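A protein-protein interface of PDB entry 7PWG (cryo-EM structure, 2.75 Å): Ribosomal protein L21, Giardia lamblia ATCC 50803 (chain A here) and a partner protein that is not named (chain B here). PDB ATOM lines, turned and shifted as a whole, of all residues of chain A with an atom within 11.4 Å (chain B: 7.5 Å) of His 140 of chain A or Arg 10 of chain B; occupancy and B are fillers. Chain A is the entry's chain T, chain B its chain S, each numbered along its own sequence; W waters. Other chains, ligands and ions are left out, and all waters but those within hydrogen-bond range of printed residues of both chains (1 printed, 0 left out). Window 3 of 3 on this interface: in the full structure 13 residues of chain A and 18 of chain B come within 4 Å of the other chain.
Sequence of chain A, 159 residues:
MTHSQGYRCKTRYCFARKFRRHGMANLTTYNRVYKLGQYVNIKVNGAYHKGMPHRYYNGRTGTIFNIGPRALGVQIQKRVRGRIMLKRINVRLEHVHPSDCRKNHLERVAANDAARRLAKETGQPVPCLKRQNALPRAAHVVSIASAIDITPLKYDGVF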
ATOM      1  N   LEU A 135     -24.332  26.210  40.465  1.00  0.00           N
ATOM      2  CA  LEU A 135     -24.146  25.009  41.260  1.00  0.00           C
ATOM      3  C   LEU A 135     -24.020  23.780  40.374  1.00  0.00           C
ATOM      4  O   LEU A 135     -24.371  23.812  39.191  1.00  0.00           O
ATOM      5  CB  LEU A 135     -25.321  24.844  42.219  1.00  0.00           C
ATOM      6  CG  LEU A 135     -25.393  25.927  43.297  1.00  0.00           C
ATOM      7  CD1 LEU A 135     -26.816  26.259  43.672  1.00  0.00           C
ATOM      8  CD2 LEU A 135     -24.607  25.489  44.519  1.00  0.00           C
ATOM      9  N   PRO A 136     -23.471  22.688  40.903  1.00  0.00           N
ATOM     10  CA  PRO A 136     -23.518  21.418  40.170  1.00  0.00           C
ATOM     11  C   PRO A 136     -24.945  20.912  40.017  1.00  0.00           C
ATOM     12  O   PRO A 136     -25.782  21.081  40.905  1.00  0.00           O
ATOM     13  CB  PRO A 136     -22.677  20.477  41.038  1.00  0.00           C
ATOM     14  CG  PRO A 136     -22.539  21.174  42.355  1.00  0.00           C
ATOM     15  CD  PRO A 136     -22.581  22.615  42.071  1.00  0.00           C
ATOM     16  N   ARG A 137     -25.207  20.254  38.884  1.00  0.00           N
ATOM     17  CA  ARG A 137     -26.555  19.812  38.543  1.00  0.00           C
ATOM     18  C   ARG A 137     -27.051  18.743  39.510  1.00  0.00           C
ATOM     19  O   ARG A 137     -26.270  17.993  40.092  1.00  0.00           O
ATOM     20  CB  ARG A 137     -26.604  19.254  37.122  1.00  0.00           C
ATOM     21  CG  ARG A 137     -25.662  19.916  36.145  1.00  0.00           C
ATOM     22  CD  ARG A 137     -25.462  19.078  34.883  1.00  0.00           C
ATOM     23  NE  ARG A 137     -24.474  19.681  33.985  1.00  0.00           N
ATOM     24  CZ  ARG A 137     -23.278  19.158  33.713  1.00  0.00           C
ATOM     25  NH1 ARG A 137     -22.913  18.004  34.252  1.00  0.00           N
ATOM     26  NH2 ARG A 137     -22.449  19.783  32.895  1.00  0.00           N
ATOM     27  N   ALA A 138     -28.371  18.663  39.649  1.00  0.00           N
ATOM     28  CA  ALA A 138     -29.029  17.693  40.509  1.00  0.00           C
ATOM     29  C   ALA A 138     -29.279  16.374  39.779  1.00  0.00           C
ATOM     30  O   ALA A 138     -29.073  16.249  38.569  1.00  0.00           O
ATOM     31  CB  ALA A 138     -30.347  18.252  41.035  1.00  0.00           C
ATOM     32  N   ALA A 139     -29.746  15.387  40.543  1.00  0.00           N
ATOM     33  CA  ALA A 139     -30.039  14.061  40.019  1.00  0.00           C
ATOM     34  C   ALA A 139     -31.341  14.053  39.228  1.00  0.00           C
ATOM     35  O   ALA A 139     -32.307  14.729  39.589  1.00  0.00           O
ATOM     36  CB  ALA A 139     -30.124  13.052  41.157  1.00  0.00           C
ATOM     37  N   HIS A 140     -31.365  13.274  38.149  1.00  0.00           N
ATOM     38  CA  HIS A 140     -32.515  13.221  37.259  1.00  0.00           C
ATOM     39  C   HIS A 140     -32.435  11.952  36.424  1.00  0.00           C
ATOM     40  O   HIS A 140     -31.404  11.286  36.369  1.00  0.00           O
ATOM     41  CB  HIS A 140     -32.568  14.455  36.362  1.00  0.00           C
ATOM     42  CG  HIS A 140     -31.298  14.702  35.616  1.00  0.00           C
ATOM     43  ND1 HIS A 140     -30.969  14.024  34.467  1.00  0.00           N
ATOM     44  CD2 HIS A 140     -30.258  15.524  35.878  1.00  0.00           C
ATOM     45  CE1 HIS A 140     -29.792  14.433  34.038  1.00  0.00           C
ATOM     46  NE2 HIS A 140     -29.337  15.343  34.878  1.00  0.00           N
ATOM     47  N   VAL A 141     -33.543  11.626  35.767  1.00  0.00           N
ATOM     48  CA  VAL A 141     -33.609  10.473  34.880  1.00  0.00           C
ATOM     49  C   VAL A 141     -33.673  10.958  33.438  1.00  0.00           C
ATOM     50  O   VAL A 141     -34.188  12.041  33.146  1.00  0.00           O
ATOM     51  CB  VAL A 141     -34.805   9.556  35.206  1.00  0.00           C
ATOM     52  CG1 VAL A 141     -34.658   8.961  36.587  1.00  0.00           C
ATOM     53  CG2 VAL A 141     -36.103  10.314  35.094  1.00  0.00           C
ATOM     54  N   VAL A 142     -33.119  10.154  32.536  1.00  0.00           N
ATOM     55  CA  VAL A 142     -33.146  10.435  31.105  1.00  0.00           C
ATOM     56  C   VAL A 142     -33.412   9.129  30.370  1.00  0.00           C
ATOM     57  O   VAL A 142     -32.932   8.069  30.780  1.00  0.00           O
ATOM     58  CB  VAL A 142     -31.834  11.100  30.617  1.00  0.00           C
ATOM     59  CG1 VAL A 142     -30.635  10.287  31.033  1.00  0.00           C
ATOM     60  CG2 VAL A 142     -31.839  11.271  29.115  1.00  0.00           C
ATOM     61  N   SER A 143     -34.190   9.205  29.296  1.00  0.00           N
ATOM     62  CA  SER A 143     -34.523   8.035  28.497  1.00  0.00           C
ATOM     63  C   SER A 143     -33.389   7.642  27.563  1.00  0.00           C
ATOM     64  O   SER A 143     -32.734   8.497  26.965  1.00  0.00           O
ATOM     65  CB  SER A 143     -35.773   8.305  27.667  1.00  0.00           C
ATOM     66  OG  SER A 143     -35.971   7.290  26.703  1.00  0.00           O
ATOM     67  N   ILE A 144     -33.183   6.333  27.414  1.00  0.00           N
ATOM     68  CA  ILE A 144     -32.270   5.804  26.406  1.00  0.00           C
ATOM     69  C   ILE A 144     -32.993   4.818  25.498  1.00  0.00           C
ATOM     70  O   ILE A 144     -32.387   3.869  24.992  1.00  0.00           O
ATOM     71  CB  ILE A 144     -31.039   5.137  27.039  1.00  0.00           C
ATOM     72  CG1 ILE A 144     -31.473   3.944  27.900  1.00  0.00           C
ATOM     73  CG2 ILE A 144     -30.218   6.155  27.805  1.00  0.00           C
ATOM     74  CD1 ILE A 144     -30.396   3.417  28.786  1.00  0.00           C
ATOM     75  N   ALA A 145     -34.283   5.038  25.269  1.00  0.00           N
ATOM     76  CA  ALA A 145     -35.007   4.193  24.326  1.00  0.00           C
ATOM     77  C   ALA A 145     -34.403   4.296  22.933  1.00  0.00           C
ATOM     78  O   ALA A 145     -34.130   3.282  22.283  1.00  0.00           O
ATOM     79  CB  ALA A 145     -36.487   4.576  24.305  1.00  0.00           C
ATOM     80  N   SER A 146     -34.152   5.513  22.477  1.00  0.00           N
ATOM     81  CA  SER A 146     -33.557   5.774  21.170  1.00  0.00           C
ATOM     82  C   SER A 146     -32.154   6.327  21.387  1.00  0.00           C
ATOM     83  O   SER A 146     -31.987   7.510  21.686  1.00  0.00           O
ATOM     84  CB  SER A 146     -34.427   6.743  20.378  1.00  0.00           C
ATOM     85  OG  SER A 146     -33.799   7.118  19.172  1.00  0.00           O
ATOM     86  N   ALA A 147     -31.149   5.477  21.224  1.00  0.00           N
ATOM     87  CA  ALA A 147     -29.757   5.844  21.429  1.00  0.00           C
ATOM     88  C   ALA A 147     -28.966   5.595  20.154  1.00  0.00           C
ATOM     89  O   ALA A 147     -29.150   4.568  19.495  1.00  0.00           O
ATOM     90  CB  ALA A 147     -29.152   5.056  22.583  1.00  0.00           C
ATOM     91  N   ILE A 148     -28.095   6.545  19.805  1.00  0.00           N
ATOM     92  CA  ILE A 148     -27.279   6.478  18.597  1.00  0.00           C
ATOM     93  C   ILE A 148     -25.915   5.910  18.955  1.00  0.00           C
ATOM     94  O   ILE A 148     -25.378   6.161  20.039  1.00  0.00           O
ATOM     95  CB  ILE A 148     -27.138   7.860  17.922  1.00  0.00           C
ATOM     96  CG1 ILE A 148     -28.447   8.636  18.013  1.00  0.00           C
ATOM     97  CG2 ILE A 148     -26.772   7.706  16.469  1.00  0.00           C
ATOM     98  CD1 ILE A 148     -29.602   7.953  17.324  1.00  0.00           C
ATOM     99  N   ILE A 150     -22.114   5.724  17.797  1.00  0.00           N
ATOM    100  CA  ILE A 150     -21.050   6.260  16.974  1.00  0.00           C
ATOM    101  C   ILE A 150     -19.733   5.590  17.336  1.00  0.00           C
ATOM    102  O   ILE A 150     -19.624   4.859  18.313  1.00  0.00           O
ATOM    103  CB  ILE A 150     -20.947   7.791  17.074  1.00  0.00           C
ATOM    104  CG1 ILE A 150     -20.818   8.265  18.511  1.00  0.00           C
ATOM    105  CG2 ILE A 150     -22.142   8.440  16.422  1.00  0.00           C
ATOM    106  CD1 ILE A 150     -20.740   9.768  18.593  1.00  0.00           C
ATOM    107  N   TYR B   8     -22.366   6.713  27.916  1.00  0.00           N
ATOM    108  CA  TYR B   8     -23.485   7.468  27.361  1.00  0.00           C
ATOM    109  C   TYR B   8     -23.279   8.955  27.598  1.00  0.00           C
ATOM    110  O   TYR B   8     -22.813   9.361  28.661  1.00  0.00           O
ATOM    111  CB  TYR B   8     -24.802   7.063  28.017  1.00  0.00           C
ATOM    112  CG  TYR B   8     -25.294   5.681  27.707  1.00  0.00           C
ATOM    113  CD1 TYR B   8     -24.760   4.572  28.337  1.00  0.00           C
ATOM    114  CD2 TYR B   8     -26.327   5.492  26.819  1.00  0.00           C
ATOM    115  CE1 TYR B   8     -25.223   3.322  28.063  1.00  0.00           C
ATOM    116  CE2 TYR B   8     -26.791   4.251  26.545  1.00  0.00           C
ATOM    117  CZ  TYR B   8     -26.244   3.168  27.170  1.00  0.00           C
ATOM    118  OH  TYR B   8     -26.735   1.921  26.881  1.00  0.00           O
ATOM    119  N   GLY B   9     -23.654   9.775  26.625  1.00  0.00           N
ATOM    120  CA  GLY B   9     -23.461  11.207  26.742  1.00  0.00           C
ATOM    121  C   GLY B   9     -24.494  11.935  25.919  1.00  0.00           C
ATOM    122  O   GLY B   9     -25.216  11.331  25.129  1.00  0.00           O
ATOM    123  N   ARG B  10     -24.570  13.248  26.124  1.00  0.00           N
ATOM    124  CA  ARG B  10     -25.535  14.067  25.402  1.00  0.00           C
ATOM    125  C   ARG B  10     -25.235  15.536  25.631  1.00  0.00           C
ATOM    126  O   ARG B  10     -24.680  15.914  26.662  1.00  0.00           O
ATOM    127  CB  ARG B  10     -26.974  13.770  25.830  1.00  0.00           C
ATOM    128  CG  ARG B  10     -27.284  14.160  27.248  1.00  0.00           C
ATOM    129  CD  ARG B  10     -28.731  14.477  27.409  1.00  0.00           C
ATOM    130  NE  ARG B  10     -29.012  14.915  28.763  1.00  0.00           N
ATOM    131  CZ  ARG B  10     -30.224  15.129  29.259  1.00  0.00           C
ATOM    132  NH1 ARG B  10     -30.347  15.526  30.510  1.00  0.00           N
ATOM    133  NH2 ARG B  10     -31.299  14.949  28.513  1.00  0.00           N
ATOM    134  N   ARG B  11     -25.616  16.352  24.659  1.00  0.00           N
ATOM    135  CA  ARG B  11     -25.553  17.795  24.803  1.00  0.00           C
ATOM    136  C   ARG B  11     -26.510  18.258  25.894  1.00  0.00           C
ATOM    137  O   ARG B  11     -27.557  17.656  26.126  1.00  0.00           O
ATOM    138  CB  ARG B  11     -25.892  18.460  23.473  1.00  0.00           C
ATOM    139  CG  ARG B  11     -26.147  19.933  23.536  1.00  0.00           C
ATOM    140  CD  ARG B  11     -26.229  20.515  22.162  1.00  0.00           C
ATOM    141  NE  ARG B  11     -24.959  20.391  21.463  1.00  0.00           N
ATOM    142  CZ  ARG B  11     -23.995  21.304  21.495  1.00  0.00           C
ATOM    143  NH1 ARG B  11     -22.869  21.101  20.828  1.00  0.00           N
ATOM    144  NH2 ARG B  11     -24.153  22.426  22.179  1.00  0.00           N
ATOM    145  N   LEU B  12     -26.127  19.323  26.587  1.00  0.00           N
ATOM    146  CA  LEU B  12     -27.003  19.896  27.591  1.00  0.00           C
ATOM    147  C   LEU B  12     -28.284  20.399  26.931  1.00  0.00           C
ATOM    148  O   LEU B  12     -28.230  21.029  25.871  1.00  0.00           O
ATOM    149  CB  LEU B  12     -26.302  21.033  28.329  1.00  0.00           C
ATOM    150  CG  LEU B  12     -25.300  20.568  29.380  1.00  0.00           C
ATOM    151  CD1 LEU B  12     -24.412  21.714  29.841  1.00  0.00           C
ATOM    152  CD2 LEU B  12     -26.032  19.933  30.542  1.00  0.00           C
ATOM    153  N   PRO B  13     -29.446  20.124  27.517  1.00  0.00           N
ATOM    154  CA  PRO B  13     -30.712  20.494  26.875  1.00  0.00           C
ATOM    155  C   PRO B  13     -31.008  21.980  26.967  1.00  0.00           C
ATOM    156  O   PRO B  13     -30.777  22.623  27.994  1.00  0.00           O
ATOM    157  CB  PRO B  13     -31.748  19.679  27.656  1.00  0.00           C
ATOM    158  CG  PRO B  13     -31.108  19.430  28.981  1.00  0.00           C
ATOM    159  CD  PRO B  13     -29.647  19.323  28.737  1.00  0.00           C
ATOM    160  N   PRO B  18     -35.198  20.747  23.407  1.00  0.00           N
ATOM    161  CA  PRO B  18     -35.459  19.910  24.579  1.00  0.00           C
ATOM    162  C   PRO B  18     -35.382  18.438  24.208  1.00  0.00           C
ATOM    163  O   PRO B  18     -35.805  18.032  23.123  1.00  0.00           O
ATOM    164  CB  PRO B  18     -36.878  20.311  24.990  1.00  0.00           C
ATOM    165  CG  PRO B  18     -37.516  20.707  23.713  1.00  0.00           C
ATOM    166  CD  PRO B  18     -36.433  21.356  22.884  1.00  0.00           C
ATOM    167  N   GLU B  19     -34.853  17.638  25.129  1.00  0.00           N
ATOM    168  CA  GLU B  19     -34.556  16.227  24.903  1.00  0.00           C
ATOM    169  C   GLU B  19     -33.577  16.040  23.745  1.00  0.00           C
ATOM    170  O   GLU B  19     -33.971  15.570  22.671  1.00  0.00           O
ATOM    171  CB  GLU B  19     -35.842  15.431  24.657  1.00  0.00           C
ATOM    172  N   PRO B  20     -32.302  16.390  23.924  1.00  0.00           N
ATOM    173  CA  PRO B  20     -31.294  16.095  22.900  1.00  0.00           C
ATOM    174  C   PRO B  20     -31.055  14.597  22.757  1.00  0.00           C
ATOM    175  O   PRO B  20     -31.444  13.788  23.596  1.00  0.00           O
ATOM    176  CB  PRO B  20     -30.038  16.798  23.420  1.00  0.00           C
ATOM    177  CG  PRO B  20     -30.458  17.568  24.629  1.00  0.00           C
ATOM    178  CD  PRO B  20     -31.697  16.962  25.136  1.00  0.00           C
ATOM    179  N   GLU B  21     -30.376  14.237  21.669  1.00  0.00           N
ATOM    180  CA  GLU B  21     -30.075  12.842  21.376  1.00  0.00           C
ATOM    181  C   GLU B  21     -29.029  12.276  22.336  1.00  0.00           C
ATOM    182  O   GLU B  21     -28.210  12.998  22.902  1.00  0.00           O
ATOM    183  CB  GLU B  21     -29.587  12.695  19.940  1.00  0.00           C
ATOM    184  N   VAL B  22     -29.061  10.959  22.507  1.00  0.00           N
ATOM    185  CA  VAL B  22     -28.148  10.241  23.386  1.00  0.00           C
ATOM    186  C   VAL B  22     -27.205   9.428  22.513  1.00  0.00           C
ATOM    187  O   VAL B  22     -27.630   8.833  21.518  1.00  0.00           O
ATOM    188  CB  VAL B  22     -28.925   9.365  24.387  1.00  0.00           C
ATOM    189  CG1 VAL B  22     -28.015   8.432  25.131  1.00  0.00           C
ATOM    190  CG2 VAL B  22     -29.664  10.248  25.375  1.00  0.00           C
ATOM    191  N   PHE B  23     -25.918   9.464  22.838  1.00  0.00           N
ATOM    192  CA  PHE B  23     -24.882   8.773  22.082  1.00  0.00           C
ATOM    193  C   PHE B  23     -24.138   7.827  23.006  1.00  0.00           C
ATOM    194  O   PHE B  23     -23.786   8.204  24.120  1.00  0.00           O
ATOM    195  CB  PHE B  23     -23.894   9.754  21.462  1.00  0.00           C
ATOM    196  CG  PHE B  23     -24.534  10.802  20.622  1.00  0.00           C
ATOM    197  CD1 PHE B  23     -24.923  10.521  19.335  1.00  0.00           C
ATOM    198  CD2 PHE B  23     -24.744  12.071  21.112  1.00  0.00           C
ATOM    199  CE1 PHE B  23     -25.509  11.471  18.566  1.00  0.00           C
ATOM    200  CE2 PHE B  23     -25.335  13.014  20.342  1.00  0.00           C
ATOM    201  CZ  PHE B  23     -25.725  12.712  19.069  1.00  0.00           C
ATOM    202  N   PHE B  39     -14.047   9.510  25.699  1.00  0.00           N
ATOM    203  CA  PHE B  39     -15.386   9.709  25.158  1.00  0.00           C
ATOM    204  C   PHE B  39     -15.595  11.143  24.698  1.00  0.00           C
ATOM    205  O   PHE B  39     -16.279  11.383  23.700  1.00  0.00           O
ATOM    206  CB  PHE B  39     -16.442   9.324  26.197  1.00  0.00           C
ATOM    207  CG  PHE B  39     -17.855   9.564  25.743  1.00  0.00           C
ATOM    208  CD1 PHE B  39     -18.542   8.601  25.021  1.00  0.00           C
ATOM    209  CD2 PHE B  39     -18.490  10.763  26.011  1.00  0.00           C
ATOM    210  CE1 PHE B  39     -19.830   8.831  24.591  1.00  0.00           C
ATOM    211  CE2 PHE B  39     -19.775  10.987  25.591  1.00  0.00           C
ATOM    212  CZ  PHE B  39     -20.444  10.022  24.881  1.00  0.00           C
ATOM    213  N   TRP B  40     -15.064  12.113  25.432  1.00  0.00           N
ATOM    214  CA  TRP B  40     -15.199  13.502  25.028  1.00  0.00           C
ATOM    215  C   TRP B  40     -14.249  13.874  23.905  1.00  0.00           C
ATOM    216  O   TRP B  40     -14.441  14.908  23.267  1.00  0.00           O
ATOM    217  CB  TRP B  40     -14.962  14.437  26.211  1.00  0.00           C
ATOM    218  CG  TRP B  40     -16.058  14.478  27.224  1.00  0.00           C
ATOM    219  CD1 TRP B  40     -15.954  14.194  28.551  1.00  0.00           C
ATOM    220  CD2 TRP B  40     -17.421  14.831  27.002  1.00  0.00           C
ATOM    221  NE1 TRP B  40     -17.158  14.353  29.167  1.00  0.00           N
ATOM    222  CE2 TRP B  40     -18.080  14.739  28.237  1.00  0.00           C
ATOM    223  CE3 TRP B  40     -18.150  15.218  25.881  1.00  0.00           C
ATOM    224  CZ2 TRP B  40     -19.427  15.023  28.380  1.00  0.00           C
ATOM    225  CZ3 TRP B  40     -19.482  15.495  26.027  1.00  0.00           C
ATOM    226  CH2 TRP B  40     -20.107  15.400  27.259  1.00  0.00           C
ATOM    227  N   LEU B  43     -16.666  12.609  20.844  1.00  0.00           N
ATOM    228  CA  LEU B  43     -17.911  13.358  20.737  1.00  0.00           C
ATOM    229  C   LEU B  43     -17.682  14.812  20.344  1.00  0.00           C
ATOM    230  O   LEU B  43     -18.614  15.466  19.877  1.00  0.00           O
ATOM    231  CB  LEU B  43     -18.682  13.282  22.056  1.00  0.00           C
ATOM    232  CG  LEU B  43     -20.168  13.584  21.888  1.00  0.00           C
ATOM    233  CD1 LEU B  43     -20.670  12.766  20.735  1.00  0.00           C
ATOM    234  CD2 LEU B  43     -20.967  13.265  23.116  1.00  0.00           C
ATOM    235  N   ILE B  49     -19.578  18.420  20.131  1.00  0.00           N
ATOM    236  CA  ILE B  49     -20.074  18.689  21.475  1.00  0.00           C
ATOM    237  C   ILE B  49     -18.869  18.677  22.403  1.00  0.00           C
ATOM    238  O   ILE B  49     -18.456  17.612  22.874  1.00  0.00           O
ATOM    239  CB  ILE B  49     -21.119  17.670  21.926  1.00  0.00           C
ATOM    240  CG1 ILE B  49     -22.268  17.595  20.932  1.00  0.00           C
ATOM    241  CG2 ILE B  49     -21.632  18.013  23.320  1.00  0.00           C
ATOM    242  CD1 ILE B  49     -23.352  16.658  21.347  1.00  0.00           C
ATOM    243  N   LYS B  50     -18.311  19.853  22.687  1.00  0.00           N
ATOM    244  CA  LYS B  50     -17.261  19.958  23.690  1.00  0.00           C
ATOM    245  C   LYS B  50     -17.774  19.478  25.043  1.00  0.00           C
ATOM    246  O   LYS B  50     -18.972  19.389  25.285  1.00  0.00           O
ATOM    247  CB  LYS B  50     -16.765  21.398  23.823  1.00  0.00           C
ATOM    248  CG  LYS B  50     -15.883  21.884  22.705  1.00  0.00           C
ATOM    249  CD  LYS B  50     -15.223  23.191  23.074  1.00  0.00           C
ATOM    250  CE  LYS B  50     -16.236  24.245  23.411  1.00  0.00           C
ATOM    251  NZ  LYS B  50     -15.590  25.514  23.801  1.00  0.00           N
ATOM    252  N   ARG B  51     -16.836  19.195  25.936  1.00  0.00           N
ATOM    253  CA  ARG B  51     -17.183  18.704  27.265  1.00  0.00           C
ATOM    254  C   ARG B  51     -17.888  19.759  28.101  1.00  0.00           C
ATOM    255  O   ARG B  51     -18.676  19.422  28.989  1.00  0.00           O
ATOM    256  CB  ARG B  51     -15.924  18.236  27.978  1.00  0.00           C
ATOM    257  CG  ARG B  51     -16.184  17.662  29.327  1.00  0.00           C
ATOM    258  CD  ARG B  51     -15.066  18.002  30.257  1.00  0.00           C
ATOM    259  NE  ARG B  51     -14.275  16.840  30.634  1.00  0.00           N
ATOM    260  CZ  ARG B  51     -13.075  16.550  30.152  1.00  0.00           C
ATOM    261  NH1 ARG B  51     -12.509  17.327  29.249  1.00  0.00           N
ATOM    262  NH2 ARG B  51     -12.438  15.470  30.571  1.00  0.00           N
ATOM    263  N   HIS B  53     -20.180  21.618  27.156  1.00  0.00           N
ATOM    264  CA  HIS B  53     -21.528  21.810  26.653  1.00  0.00           C
ATOM    265  C   HIS B  53     -22.409  20.577  26.797  1.00  0.00           C
ATOM    266  O   HIS B  53     -23.537  20.581  26.303  1.00  0.00           O
ATOM    267  CB  HIS B  53     -21.462  22.243  25.188  1.00  0.00           C
ATOM    268  CG  HIS B  53     -20.898  23.613  24.987  1.00  0.00           C
ATOM    269  ND1 HIS B  53     -19.963  23.898  24.019  1.00  0.00           N
ATOM    270  CD2 HIS B  53     -21.143  24.779  25.627  1.00  0.00           C
ATOM    271  CE1 HIS B  53     -19.656  25.179  24.070  1.00  0.00           C
ATOM    272  NE2 HIS B  53     -20.361  25.739  25.035  1.00  0.00           N
ATOM    273  N   GLY B  54     -21.934  19.530  27.471  1.00  0.00           N
ATOM    274  CA  GLY B  54     -22.665  18.288  27.574  1.00  0.00           C
ATOM    275  C   GLY B  54     -22.421  17.617  28.905  1.00  0.00           C
ATOM    276  O   GLY B  54     -21.719  18.142  29.766  1.00  0.00           O
ATOM    277  N   GLU B  55     -23.020  16.440  29.072  1.00  0.00           N
ATOM    278  CA  GLU B  55     -22.914  15.707  30.324  1.00  0.00           C
ATOM    279  C   GLU B  55     -22.887  14.213  30.052  1.00  0.00           C
ATOM    280  O   GLU B  55     -23.469  13.734  29.081  1.00  0.00           O
ATOM    281  CB  GLU B  55     -24.059  16.035  31.280  1.00  0.00           C
ATOM    282  CG  GLU B  55     -25.390  15.399  30.943  1.00  0.00           C
ATOM    283  CD  GLU B  55     -26.479  15.849  31.879  1.00  0.00           C
ATOM    284  OE1 GLU B  55     -26.289  16.878  32.548  1.00  0.00           O
ATOM    285  OE2 GLU B  55     -27.528  15.179  31.969  1.00  0.00           O
ATOM    286  N   ILE B  56     -22.211  13.489  30.933  1.00  0.00           N
ATOM    287  CA  ILE B  56     -22.040  12.049  30.822  1.00  0.00           C
ATOM    288  C   ILE B  56     -23.085  11.362  31.688  1.00  0.00           C
ATOM    289  O   ILE B  56     -23.236  11.681  32.874  1.00  0.00           O
ATOM    290  CB  ILE B  56     -20.618  11.625  31.223  1.00  0.00           C
ATOM    291  CG1 ILE B  56     -19.720  11.604  30.000  1.00  0.00           C
ATOM    292  CG2 ILE B  56     -20.611  10.250  31.872  1.00  0.00           C
ATOM    293  CD1 ILE B  56     -18.284  11.453  30.326  1.00  0.00           C
ATOM    294  N   LEU B  57     -23.803  10.421  31.094  1.00  0.00           N
ATOM    295  CA  LEU B  57     -24.898   9.766  31.787  1.00  0.00           C
ATOM    296  C   LEU B  57     -24.480   8.476  32.476  1.00  0.00           C
ATOM    297  O   LEU B  57     -25.006   8.185  33.550  1.00  0.00           O
ATOM    298  CB  LEU B  57     -26.042   9.518  30.808  1.00  0.00           C
ATOM    299  CG  LEU B  57     -26.407  10.746  29.955  1.00  0.00           C
ATOM    300  CD1 LEU B  57     -27.166  10.335  28.739  1.00  0.00           C
ATOM    301  CD2 LEU B  57     -27.199  11.775  30.733  1.00  0.00           C
HETATM  302  O   HOH W   1     -32.425  10.533  22.925  1.00  0.00           O
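The side-chain carboxylate (OE2) of Glu 55 of chain B sits close to a ring nitrogen (NE2) of His 140 of chain A (3.4 Å). OE1 of Glu 55 of chain B is in salt-bridge range of NE of Arg 137 of chain A, at 3.6 Å. The backbone NH (N) of Ile 148 of chain A sits at hydrogen-bond distance from the backbone carbonyl oxygen (O) of Val 22 of chain B (2.9 Å).
The backbone carbonyl oxygen (O) of His 53 of chain B sits at hydrogen-bond distance from the backbone NH (N) of Leu 12 of chain B (2.9 Å). The backbone NH of Leu 57 of chain B sits at hydrogen-bond distance from the backbone carbonyl oxygen of Tyr 8 of chain B (2.8 Å). OE2 of Glu 55 of chain B is in salt-bridge range of NH1 of Arg 10 of chain B. The backbone carbonyl oxygen (O) of Leu 43 of chain B sits at hydrogen-bond distance from the backbone NH (N) of Ile 49 of chain B.
NE of Arg 137 of chain A touches CD2 of Leu 12 of chain B (3.8 Å). O of Gly 54 of chain B touches NH2 of Arg 137 of chain A, at 3.6 Å. His 140 of chain A touches Arg 10 of chain B. Arg 10 of chain B touches Val 142 of chain A. CG1 of Val 142 of chain A touches CD2 of Leu 57 of chain B (3.8 Å). Val 22 of chain B touches Ser 143 of chain A (CG2 to O, 3.9 Å). Ala 147 of chain A touches Val 22 of chain B. Ile 148 of chain A touches Phe 23 of chain B (O to CA, 3.4 Å). Ile 150 of chain A touches Leu 43 of chain B.
Of chain B, only Arg 10 and Glu 55 come within 4 Å of His 140 of chain A. Of chain A, only His 140 (3.7 Å) and Val 142 (3.8 Å) come within 4 Å of Arg 10 of chain B. No residue of chain A comes within 4 Å of Pro 20 of chain B. Of the printed residues of chain A, Val 22 of chain B touches Ser 143 (3.9 Å), Ala 147 (3.7 Å) and Ile 148 (2.9 Å). Phe 23 of chain B touches just one residue of chain A: Ile 148 (3.4 Å). Of the printed residues of chain A, Gly 54 of chain B touches Arg 137 (3.6 Å). Of chain A, only Arg 137 (3.3 Å) and His 140 (3.2 Å) come within 4 Å of Glu 55 of chain B. Of the printed residues of chain B, Ser 143 of chain A touches Val 22. Of the printed residues of chain B, Val 142 of chain A touches Arg 10 and Leu 57. Of the printed residues of chain A, Leu 43 of chain B touches Ile 150 (3.7 Å). Pro 136 of chain A touches none of the printed residues of chain B. The nearest residue of chain B that does not touch His 140 of chain A is Leu 57 of chain B (5.0 Å). The nearest printed residue of chain A that does not touch Leu 57 of chain B is His 140 of chain A (5.0 Å).
Of the 23 printed residues of chain B, 8 touch a printed residue of chain A. Of the 15 printed residues of chain A, 7 touch a printed residue of chain B. Hydrophobic or aromatic side chains of chain A within 4 Å of the printed part of chain B: His 140, Val 142, Ile 148 and Ile 150. Among the printed residues, 12 pairs touch across the chains. Among the printed residues, Asp or Glu carboxylates within 4 Å of a Lys or Arg side-chain nitrogen of the other chain: Arg 137 of chain A with Glu 55 of chain B.
Water W1 lies within hydrogen-bond range of the backbone carbonyl oxygen (O) of Ser 146 of chain A (3.3 Å), the backbone NH (N) of Val 22 of chain B (3.4 Å) and the backbone carbonyl oxygen (O) of Pro 20 of chain B (3.5 Å).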
